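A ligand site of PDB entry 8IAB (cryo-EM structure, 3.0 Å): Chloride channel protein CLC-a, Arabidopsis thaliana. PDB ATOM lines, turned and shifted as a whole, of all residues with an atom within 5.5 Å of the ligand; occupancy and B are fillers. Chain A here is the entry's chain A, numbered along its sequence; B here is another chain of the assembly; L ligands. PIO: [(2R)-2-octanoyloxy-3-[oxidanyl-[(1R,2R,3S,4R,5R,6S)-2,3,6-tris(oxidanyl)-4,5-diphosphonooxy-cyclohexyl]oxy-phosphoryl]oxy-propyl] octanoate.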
ATOM      1  N   TRP A  71      11.402 -19.532  18.917  1.00  0.00           N
ATOM      2  CA  TRP A  71      10.017 -19.537  18.487  1.00  0.00           C
ATOM      3  C   TRP A  71       9.741 -18.553  17.357  1.00  0.00           C
ATOM      4  O   TRP A  71       8.683 -18.636  16.739  1.00  0.00           O
ATOM      5  CB  TRP A  71       9.084 -19.245  19.664  1.00  0.00           C
ATOM      6  CG  TRP A  71       9.311 -17.919  20.322  1.00  0.00           C
ATOM      7  CD1 TRP A  71      10.133 -17.669  21.385  1.00  0.00           C
ATOM      8  CD2 TRP A  71       8.707 -16.668  19.979  1.00  0.00           C
ATOM      9  NE1 TRP A  71      10.082 -16.337  21.714  1.00  0.00           N
ATOM     10  CE2 TRP A  71       9.204 -15.706  20.871  1.00  0.00           C
ATOM     11  CE3 TRP A  71       7.780 -16.279  19.006  1.00  0.00           C
ATOM     12  CZ2 TRP A  71       8.824 -14.365  20.818  1.00  0.00           C
ATOM     13  CZ3 TRP A  71       7.408 -14.949  18.956  1.00  0.00           C
ATOM     14  CH2 TRP A  71       7.922 -14.009  19.851  1.00  0.00           C
ATOM     15  N   ARG A  72      10.670 -17.636  17.086  1.00  0.00           N
ATOM     16  CA  ARG A  72      10.501 -16.711  15.973  1.00  0.00           C
ATOM     17  C   ARG A  72      10.830 -17.349  14.626  1.00  0.00           C
ATOM     18  O   ARG A  72      10.544 -16.746  13.584  1.00  0.00           O
ATOM     19  CB  ARG A  72      11.377 -15.479  16.175  1.00  0.00           C
ATOM     20  CG  ARG A  72      11.115 -14.735  17.470  1.00  0.00           C
ATOM     21  CD  ARG A  72      12.236 -13.751  17.751  1.00  0.00           C
ATOM     22  NE  ARG A  72      11.967 -12.957  18.952  1.00  0.00           N
ATOM     23  CZ  ARG A  72      12.365 -13.287  20.168  1.00  0.00           C
ATOM     24  NH1 ARG A  72      13.060 -14.395  20.363  1.00  0.00           N
ATOM     25  NH2 ARG A  72      12.076 -12.505  21.193  1.00  0.00           N
ATOM     26  N   PHE A  80       1.173 -17.998  16.612  1.00  0.00           N
ATOM     27  CA  PHE A  80      -0.092 -17.639  17.232  1.00  0.00           C
ATOM     28  C   PHE A  80      -0.584 -18.718  18.185  1.00  0.00           C
ATOM     29  O   PHE A  80      -1.297 -18.402  19.147  1.00  0.00           O
ATOM     30  CB  PHE A  80      -1.153 -17.363  16.160  1.00  0.00           C
ATOM     31  CG  PHE A  80      -1.128 -15.954  15.642  1.00  0.00           C
ATOM     32  CD1 PHE A  80      -0.621 -15.678  14.381  1.00  0.00           C
ATOM     33  CD2 PHE A  80      -1.622 -14.914  16.417  1.00  0.00           C
ATOM     34  CE1 PHE A  80      -0.597 -14.380  13.904  1.00  0.00           C
ATOM     35  CE2 PHE A  80      -1.605 -13.622  15.933  1.00  0.00           C
ATOM     36  CZ  PHE A  80      -1.097 -13.353  14.679  1.00  0.00           C
ATOM     37  N   ILE A  83       1.633 -17.985  21.283  1.00  0.00           N
ATOM     38  CA  ILE A  83       1.248 -16.751  21.964  1.00  0.00           C
ATOM     39  C   ILE A  83      -0.064 -16.946  22.723  1.00  0.00           C
ATOM     40  O   ILE A  83      -0.200 -16.501  23.869  1.00  0.00           O
ATOM     41  CB  ILE A  83       1.161 -15.600  20.945  1.00  0.00           C
ATOM     42  CG1 ILE A  83       2.554 -15.119  20.571  1.00  0.00           C
ATOM     43  CG2 ILE A  83       0.351 -14.424  21.477  1.00  0.00           C
ATOM     44  CD1 ILE A  83       2.567 -14.116  19.454  1.00  0.00           C
ATOM     45  N   PHE A  84      -1.027 -17.658  22.117  1.00  0.00           N
ATOM     46  CA  PHE A  84      -2.310 -17.903  22.773  1.00  0.00           C
ATOM     47  C   PHE A  84      -2.149 -18.819  23.972  1.00  0.00           C
ATOM     48  O   PHE A  84      -2.774 -18.602  25.011  1.00  0.00           O
ATOM     49  CB  PHE A  84      -3.294 -18.497  21.762  1.00  0.00           C
ATOM     50  CG  PHE A  84      -4.408 -19.305  22.378  1.00  0.00           C
ATOM     51  CD1 PHE A  84      -4.405 -20.690  22.307  1.00  0.00           C
ATOM     52  CD2 PHE A  84      -5.469 -18.677  23.011  1.00  0.00           C
ATOM     53  CE1 PHE A  84      -5.418 -21.429  22.873  1.00  0.00           C
ATOM     54  CE2 PHE A  84      -6.490 -19.412  23.581  1.00  0.00           C
ATOM     55  CZ  PHE A  84      -6.460 -20.786  23.506  1.00  0.00           C
ATOM     56  N   LYS A  86       0.607 -19.132  25.717  1.00  0.00           N
ATOM     57  CA  LYS A  86       1.357 -18.395  26.726  1.00  0.00           C
ATOM     58  C   LYS A  86       0.417 -17.628  27.652  1.00  0.00           C
ATOM     59  O   LYS A  86       0.629 -17.599  28.864  1.00  0.00           O
ATOM     60  CB  LYS A  86       2.321 -17.422  26.066  1.00  0.00           C
ATOM     61  CG  LYS A  86       3.761 -17.870  26.049  1.00  0.00           C
ATOM     62  CD  LYS A  86       4.685 -16.688  25.818  1.00  0.00           C
ATOM     63  CE  LYS A  86       4.341 -15.949  24.528  1.00  0.00           C
ATOM     64  NZ  LYS A  86       5.230 -14.789  24.320  1.00  0.00           N
ATOM     65  N   TRP A  87      -0.605 -16.995  27.093  1.00  0.00           N
ATOM     66  CA  TRP A  87      -1.507 -16.161  27.882  1.00  0.00           C
ATOM     67  C   TRP A  87      -2.662 -16.954  28.458  1.00  0.00           C
ATOM     68  O   TRP A  87      -3.323 -16.486  29.390  1.00  0.00           O
ATOM     69  CB  TRP A  87      -2.015 -15.008  27.034  1.00  0.00           C
ATOM     70  CG  TRP A  87      -0.966 -13.968  26.830  1.00  0.00           C
ATOM     71  CD1 TRP A  87      -0.030 -13.932  25.850  1.00  0.00           C
ATOM     72  CD2 TRP A  87      -0.710 -12.841  27.669  1.00  0.00           C
ATOM     73  NE1 TRP A  87       0.778 -12.844  26.004  1.00  0.00           N
ATOM     74  CE2 TRP A  87       0.387 -12.151  27.117  1.00  0.00           C
ATOM     75  CE3 TRP A  87      -1.314 -12.334  28.818  1.00  0.00           C
ATOM     76  CZ2 TRP A  87       0.886 -10.983  27.683  1.00  0.00           C
ATOM     77  CZ3 TRP A  87      -0.812 -11.183  29.381  1.00  0.00           C
ATOM     78  CH2 TRP A  87       0.275 -10.514  28.807  1.00  0.00           C
ATOM     79  N   ASP A 243       9.843 -18.947  32.864  1.00  0.00           N
ATOM     80  CA  ASP A 243       8.805 -17.930  32.745  1.00  0.00           C
ATOM     81  C   ASP A 243       7.527 -18.342  33.455  1.00  0.00           C
ATOM     82  O   ASP A 243       6.840 -17.497  34.029  1.00  0.00           O
ATOM     83  CB  ASP A 243       8.516 -17.632  31.275  1.00  0.00           C
ATOM     84  CG  ASP A 243       9.686 -16.976  30.576  1.00  0.00           C
ATOM     85  OD1 ASP A 243      10.596 -16.497  31.272  1.00  0.00           O
ATOM     86  OD2 ASP A 243       9.685 -16.957  29.326  1.00  0.00           O
ATOM     87  N   ARG A 276      12.704  -9.566  32.098  1.00  0.00           N
ATOM     88  CA  ARG A 276      12.482  -8.665  30.977  1.00  0.00           C
ATOM     89  C   ARG A 276      11.095  -8.054  31.110  1.00  0.00           C
ATOM     90  O   ARG A 276      10.304  -8.433  31.965  1.00  0.00           O
ATOM     91  CB  ARG A 276      12.629  -9.380  29.633  1.00  0.00           C
ATOM     92  CG  ARG A 276      11.676 -10.528  29.426  1.00  0.00           C
ATOM     93  CD  ARG A 276      12.236 -11.505  28.418  1.00  0.00           C
ATOM     94  NE  ARG A 276      11.225 -12.482  28.000  1.00  0.00           N
ATOM     95  CZ  ARG A 276      11.021 -13.635  28.608  1.00  0.00           C
ATOM     96  NH1 ARG A 276      10.085 -14.469  28.164  1.00  0.00           N
ATOM     97  NH2 ARG A 276      11.748 -13.974  29.668  1.00  0.00           N
ATOM     98  N   ALA A 278       8.638  -8.173  28.892  1.00  0.00           N
ATOM     99  CA  ALA A 278       7.572  -9.040  28.422  1.00  0.00           C
ATOM    100  C   ALA A 278       7.130 -10.023  29.492  1.00  0.00           C
ATOM    101  O   ALA A 278       5.949 -10.374  29.573  1.00  0.00           O
ATOM    102  CB  ALA A 278       8.018  -9.788  27.168  1.00  0.00           C
ATOM    103  N   TRP A 281       4.782  -8.192  32.162  1.00  0.00           N
ATOM    104  CA  TRP A 281       3.384  -7.968  31.852  1.00  0.00           C
ATOM    105  C   TRP A 281       2.543  -9.234  31.907  1.00  0.00           C
ATOM    106  O   TRP A 281       1.356  -9.167  32.229  1.00  0.00           O
ATOM    107  CB  TRP A 281       3.273  -7.308  30.470  1.00  0.00           C
ATOM    108  CG  TRP A 281       1.876  -6.984  29.957  1.00  0.00           C
ATOM    109  CD1 TRP A 281       1.387  -7.261  28.718  1.00  0.00           C
ATOM    110  CD2 TRP A 281       0.816  -6.291  30.647  1.00  0.00           C
ATOM    111  NE1 TRP A 281       0.101  -6.817  28.598  1.00  0.00           N
ATOM    112  CE2 TRP A 281      -0.275  -6.211  29.763  1.00  0.00           C
ATOM    113  CE3 TRP A 281       0.682  -5.738  31.928  1.00  0.00           C
ATOM    114  CZ2 TRP A 281      -1.476  -5.607  30.112  1.00  0.00           C
ATOM    115  CZ3 TRP A 281      -0.511  -5.138  32.272  1.00  0.00           C
ATOM    116  CH2 TRP A 281      -1.575  -5.079  31.364  1.00  0.00           C
ATOM    117  N   ARG A 282       3.145 -10.392  31.622  1.00  0.00           N
ATOM    118  CA  ARG A 282       2.450 -11.661  31.842  1.00  0.00           C
ATOM    119  C   ARG A 282       2.311 -11.981  33.322  1.00  0.00           C
ATOM    120  O   ARG A 282       1.309 -12.558  33.737  1.00  0.00           O
ATOM    121  CB  ARG A 282       3.183 -12.803  31.130  1.00  0.00           C
ATOM    122  CG  ARG A 282       2.436 -13.361  29.944  1.00  0.00           C
ATOM    123  CD  ARG A 282       3.004 -14.686  29.476  1.00  0.00           C
ATOM    124  NE  ARG A 282       4.473 -14.726  29.446  1.00  0.00           N
ATOM    125  CZ  ARG A 282       5.230 -14.161  28.514  1.00  0.00           C
ATOM    126  NH1 ARG A 282       4.695 -13.492  27.506  1.00  0.00           N
ATOM    127  NH2 ARG A 282       6.552 -14.279  28.590  1.00  0.00           N
ATOM    128  N   PHE A 285      -0.443  -9.849  34.745  1.00  0.00           N
ATOM    129  CA  PHE A 285      -1.753 -10.348  34.359  1.00  0.00           C
ATOM    130  C   PHE A 285      -2.187 -11.501  35.255  1.00  0.00           C
ATOM    131  O   PHE A 285      -3.369 -11.627  35.586  1.00  0.00           O
ATOM    132  CB  PHE A 285      -1.732 -10.776  32.897  1.00  0.00           C
ATOM    133  CG  PHE A 285      -2.923 -11.588  32.468  1.00  0.00           C
ATOM    134  CD1 PHE A 285      -2.753 -12.879  31.994  1.00  0.00           C
ATOM    135  CD2 PHE A 285      -4.193 -11.046  32.514  1.00  0.00           C
ATOM    136  CE1 PHE A 285      -3.848 -13.622  31.590  1.00  0.00           C
ATOM    137  CE2 PHE A 285      -5.288 -11.789  32.110  1.00  0.00           C
ATOM    138  CZ  PHE A 285      -5.111 -13.082  31.649  1.00  0.00           C
ATOM    139  N   PHE B 547      -7.735  -4.623  32.494  1.00  0.00           N
ATOM    140  CA  PHE B 547      -8.462  -5.281  31.420  1.00  0.00           C
ATOM    141  C   PHE B 547      -8.437  -4.471  30.133  1.00  0.00           C
ATOM    142  O   PHE B 547      -8.301  -5.049  29.048  1.00  0.00           O
ATOM    143  CB  PHE B 547      -9.906  -5.538  31.852  1.00  0.00           C
ATOM    144  CG  PHE B 547     -10.733  -6.280  30.843  1.00  0.00           C
ATOM    145  CD1 PHE B 547     -11.827  -5.673  30.245  1.00  0.00           C
ATOM    146  CD2 PHE B 547     -10.399  -7.578  30.484  1.00  0.00           C
ATOM    147  CE1 PHE B 547     -12.583  -6.356  29.311  1.00  0.00           C
ATOM    148  CE2 PHE B 547     -11.155  -8.260  29.550  1.00  0.00           C
ATOM    149  CZ  PHE B 547     -12.251  -7.644  28.963  1.00  0.00           C
ATOM    150  N   LEU B 550      -4.903  -4.373  28.591  1.00  0.00           N
ATOM    151  CA  LEU B 550      -4.581  -5.619  27.917  1.00  0.00           C
ATOM    152  C   LEU B 550      -5.018  -5.596  26.469  1.00  0.00           C
ATOM    153  O   LEU B 550      -4.264  -5.986  25.571  1.00  0.00           O
ATOM    154  CB  LEU B 550      -5.256  -6.793  28.630  1.00  0.00           C
ATOM    155  CG  LEU B 550      -4.506  -7.586  29.677  1.00  0.00           C
ATOM    156  CD1 LEU B 550      -5.501  -8.434  30.419  1.00  0.00           C
ATOM    157  CD2 LEU B 550      -3.438  -8.448  29.023  1.00  0.00           C
ATOM    158  N   ILE B 551      -6.253  -5.144  26.219  1.00  0.00           N
ATOM    159  CA  ILE B 551      -6.808  -5.156  24.875  1.00  0.00           C
ATOM    160  C   ILE B 551      -6.157  -4.084  24.007  1.00  0.00           C
ATOM    161  O   ILE B 551      -5.849  -4.316  22.842  1.00  0.00           O
ATOM    162  CB  ILE B 551      -8.334  -4.990  24.944  1.00  0.00           C
ATOM    163  CG1 ILE B 551      -8.931  -6.066  25.864  1.00  0.00           C
ATOM    164  CG2 ILE B 551      -8.960  -5.091  23.568  1.00  0.00           C
ATOM    165  CD1 ILE B 551     -10.426  -6.000  26.000  1.00  0.00           C
ATOM    166  N   LYS B 553      -3.133  -2.668  24.252  1.00  0.00           N
ATOM    167  CA  LYS B 553      -1.784  -3.029  23.861  1.00  0.00           C
ATOM    168  C   LYS B 553      -1.780  -4.169  22.837  1.00  0.00           C
ATOM    169  O   LYS B 553      -0.892  -4.212  21.984  1.00  0.00           O
ATOM    170  CB  LYS B 553      -0.974  -3.435  25.093  1.00  0.00           C
ATOM    171  CG  LYS B 553       0.515  -3.559  24.864  1.00  0.00           C
ATOM    172  CD  LYS B 553       1.147  -4.540  25.833  1.00  0.00           C
ATOM    173  CE  LYS B 553       2.658  -4.434  25.826  1.00  0.00           C
ATOM    174  NZ  LYS B 553       3.221  -4.754  24.484  1.00  0.00           N
ATOM    175  N   THR B 554      -2.768  -5.060  22.901  1.00  0.00           N
ATOM    176  CA  THR B 554      -2.816  -6.187  21.970  1.00  0.00           C
ATOM    177  C   THR B 554      -3.256  -5.729  20.585  1.00  0.00           C
ATOM    178  O   THR B 554      -2.670  -6.133  19.581  1.00  0.00           O
ATOM    179  CB  THR B 554      -3.757  -7.263  22.514  1.00  0.00           C
ATOM    180  OG1 THR B 554      -3.355  -7.617  23.838  1.00  0.00           O
ATOM    181  CG2 THR B 554      -3.730  -8.493  21.642  1.00  0.00           C
ATOM    182  N   ASP B 557      -0.340  -3.406  19.153  1.00  0.00           N
ATOM    183  CA  ASP B 557       0.873  -4.085  18.691  1.00  0.00           C
ATOM    184  C   ASP B 557       0.672  -4.839  17.378  1.00  0.00           C
ATOM    185  O   ASP B 557       1.665  -5.252  16.779  1.00  0.00           O
ATOM    186  CB  ASP B 557       1.362  -5.068  19.758  1.00  0.00           C
ATOM    187  CG  ASP B 557       2.416  -4.457  20.663  1.00  0.00           C
ATOM    188  OD1 ASP B 557       3.092  -3.501  20.247  1.00  0.00           O
ATOM    189  OD2 ASP B 557       2.564  -4.942  21.802  1.00  0.00           O
ATOM    190  N   SER B 558      -0.571  -5.026  16.929  1.00  0.00           N
ATOM    191  CA  SER B 558      -0.834  -5.734  15.687  1.00  0.00           C
ATOM    192  C   SER B 558      -0.716  -4.850  14.459  1.00  0.00           C
ATOM    193  O   SER B 558      -0.758  -5.372  13.346  1.00  0.00           O
ATOM    194  CB  SER B 558      -2.232  -6.358  15.738  1.00  0.00           C
ATOM    195  OG  SER B 558      -2.284  -7.402  16.693  1.00  0.00           O
ATOM    196  N   ALA B 578      16.614  -5.891  22.679  1.00  0.00           N
ATOM    197  CA  ALA B 578      16.978  -6.973  23.588  1.00  0.00           C
ATOM    198  C   ALA B 578      17.131  -8.313  22.867  1.00  0.00           C
ATOM    199  O   ALA B 578      18.011  -9.096  23.214  1.00  0.00           O
ATOM    200  CB  ALA B 578      15.930  -7.098  24.701  1.00  0.00           C
ATOM    201  N   ASN B 579      16.298  -8.577  21.881  1.00  0.00           N
ATOM    202  CA  ASN B 579      16.338  -9.879  21.257  1.00  0.00           C
ATOM    203  C   ASN B 579      16.829  -9.786  19.810  1.00  0.00           C
ATOM    204  O   ASN B 579      16.443  -8.858  19.091  1.00  0.00           O
ATOM    205  CB  ASN B 579      14.957 -10.544  21.261  1.00  0.00           C
ATOM    206  CG  ASN B 579      14.490 -10.881  22.660  1.00  0.00           C
ATOM    207  OD1 ASN B 579      15.009 -11.793  23.297  1.00  0.00           O
ATOM    208  ND2 ASN B 579      13.509 -10.136  23.148  1.00  0.00           N
HETATM  209  C1  PIO L   1       6.293 -10.816  23.524  1.00  0.00           C
HETATM  210  O1  PIO L   1       5.146 -11.588  23.375  1.00  0.00           O
HETATM  211  P1  PIO L   1       3.820 -11.308  24.272  1.00  0.00           P
HETATM  212  C2  PIO L   1       6.312  -9.833  22.369  1.00  0.00           C
HETATM  213  O2  PIO L   1       6.215 -10.582  21.188  1.00  0.00           O
HETATM  214  C3  PIO L   1       7.609  -9.060  22.328  1.00  0.00           C
HETATM  215  O3  PIO L   1       7.604  -8.298  21.154  1.00  0.00           O
HETATM  216  C4  PIO L   1       8.820  -9.984  22.265  1.00  0.00           C
HETATM  217  O4  PIO L   1       9.948  -9.182  22.404  1.00  0.00           O
HETATM  218  P4  PIO L   1      10.843  -8.871  21.075  1.00  0.00           P
HETATM  219  C5  PIO L   1       8.801 -11.047  23.376  1.00  0.00           C
HETATM  220  O5  PIO L   1       9.781 -12.005  23.116  1.00  0.00           O
HETATM  221  P5  PIO L   1      10.664 -12.580  24.349  1.00  0.00           P
HETATM  222  C6  PIO L   1       7.468 -11.767  23.420  1.00  0.00           C
HETATM  223  O6  PIO L   1       7.453 -12.608  24.537  1.00  0.00           O
HETATM  224  O11 PIO L   1       3.715 -12.371  25.300  1.00  0.00           O
HETATM  225  O12 PIO L   1       3.909  -9.971  24.940  1.00  0.00           O
HETATM  226  O13 PIO L   1       2.519 -11.309  23.302  1.00  0.00           O
HETATM  227  C1A PIO L   1       0.130  -9.827  19.639  1.00  0.00           C
HETATM  228  O1A PIO L   1      -0.267  -8.945  18.958  1.00  0.00           O
HETATM  229  C1B PIO L   1      -0.910  -9.652  24.790  1.00  0.00           C
HETATM  230  O1B PIO L   1      -1.002  -8.750  25.529  1.00  0.00           O
HETATM  231  C1C PIO L   1       2.336 -10.162  22.525  1.00  0.00           C
HETATM  232  C2A PIO L   1      -0.414 -11.227  19.432  1.00  0.00           C
HETATM  233  C2B PIO L   1      -2.014 -10.699  24.693  1.00  0.00           C
HETATM  234  C2C PIO L   1       0.991 -10.155  21.835  1.00  0.00           C
HETATM  235  O2C PIO L   1       1.115  -9.552  20.580  1.00  0.00           O
HETATM  236  C3A PIO L   1      -1.906 -11.215  19.149  1.00  0.00           C
HETATM  237  C3B PIO L   1      -3.094 -10.277  25.667  1.00  0.00           C
HETATM  238  C3C PIO L   1       0.061  -9.327  22.710  1.00  0.00           C
HETATM  239  O3C PIO L   1       0.217  -9.766  24.020  1.00  0.00           O
HETATM  240  O41 PIO L   1      11.973  -7.967  21.477  1.00  0.00           O
HETATM  241  O42 PIO L   1      11.397 -10.130  20.487  1.00  0.00           O
HETATM  242  O43 PIO L   1       9.988  -8.201  20.049  1.00  0.00           O
HETATM  243  C4A PIO L   1      -2.531 -12.563  19.530  1.00  0.00           C
HETATM  244  C4B PIO L   1      -4.264 -11.226  25.594  1.00  0.00           C
HETATM  245  O51 PIO L   1      11.748 -13.490  23.865  1.00  0.00           O
HETATM  246  O52 PIO L   1      11.230 -11.419  25.097  1.00  0.00           O
HETATM  247  O53 PIO L   1       9.788 -13.389  25.244  1.00  0.00           O
HETATM  248  C5A PIO L   1      -3.050 -12.493  20.950  1.00  0.00           C
HETATM  249  C5B PIO L   1      -4.740 -11.464  27.028  1.00  0.00           C
HETATM  250  C6A PIO L   1      -4.000 -13.642  21.280  1.00  0.00           C
HETATM  251  C6B PIO L   1      -5.978 -10.627  27.325  1.00  0.00           C
HETATM  252  C7A PIO L   1      -4.110 -13.734  22.802  1.00  0.00           C
HETATM  253  C7B PIO L   1      -7.022 -11.538  27.970  1.00  0.00           C
HETATM  254  C8A PIO L   1      -5.119 -14.773  23.242  1.00  0.00           C
HETATM  255  C8B PIO L   1      -8.268 -10.723  28.333  1.00  0.00           C
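The guanidinium group (NH2) of Arg 72 sits close to the side-chain amide nitrogen (ND2) of Asn 579 of chain B (3.4 Å).
NH1 of Arg 276 lies within salt-bridge range of OD2 of Asp 243 (2.8 Å).
O of Thr 554 of chain B is in hydrogen-bond range of OG of Ser 558 of chain B.
The side-chain hydroxyl (OG1) of Thr 554 of chain B lies within hydrogen-bond range of the backbone carbonyl oxygen (O) of Leu 550 of chain B (2.5 Å).
CZ2 of Trp 71 touches O5 of the ligand, at 3.4 Å.
Phe 80 touches the ligand (CE2 to C4A, 3.9 Å).
CG2 of Ile 83 touches C2A of the ligand, 3.9 Å away.
CD2 of Phe 84 touches C8A of the ligand (3.9 Å).
Ala 278 touches the ligand (CB to O6, 3.9 Å).
Trp 281 touches the ligand.
Phe 547 of chain B touches the ligand.
CD2 of Leu 550 of chain B touches C6B of the ligand, 3.8 Å away.
Hydrophobic or aromatic side chains within 4 Å of the ligand: Trp 71, Phe 80, Ile 83, Phe 84, Trp 87, Ala 278, Phe 547 of chain B and Leu 550 of chain B.
16 residues have an atom within 4 Å of the ligand: Trp 71, Arg 72, Phe 80, Ile 83, Phe 84, Lys 86, Trp 87, Arg 276, Ala 278, Trp 281, Arg 282, Phe 547 of chain B, Leu 550 of chain B, Thr 554 of chain B, Ser 558 of chain B and Asn 579 of chain B.
The nearest printed residue that does not touch the ligand is Asp 557 of chain B (4.3 Å).
O42 of the ligand lies within salt-bridge range of NH2 of Arg 72, 2.6 Å away.
An oxygen (O11) of the ligand is in salt-bridge range of the guanidinium group of Arg 282 (2.7 Å).
NZ of Lys 86 lies within salt-bridge range of O11 of the ligand (3.0 Å).
NE1 of Trp 87 lies within hydrogen-bond range of O11 of the ligand (3.1 Å).
The guanidinium group (NE) of Arg 276 is in salt-bridge range of an oxygen (O52) of the ligand (3.1 Å).
An oxygen (O1B) of the ligand lies within hydrogen-bond range of the side-chain hydroxyl of Thr 554 of chain B (3.1 Å).
ND2 of Asn 579 of chain B is in hydrogen-bond range of O41 of the ligand, at 3.1 Å.
The side-chain hydroxyl of Ser 558 of chain B sits at hydrogen-bond distance from an oxygen (O1A) of the ligand, at 3.4 Å.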
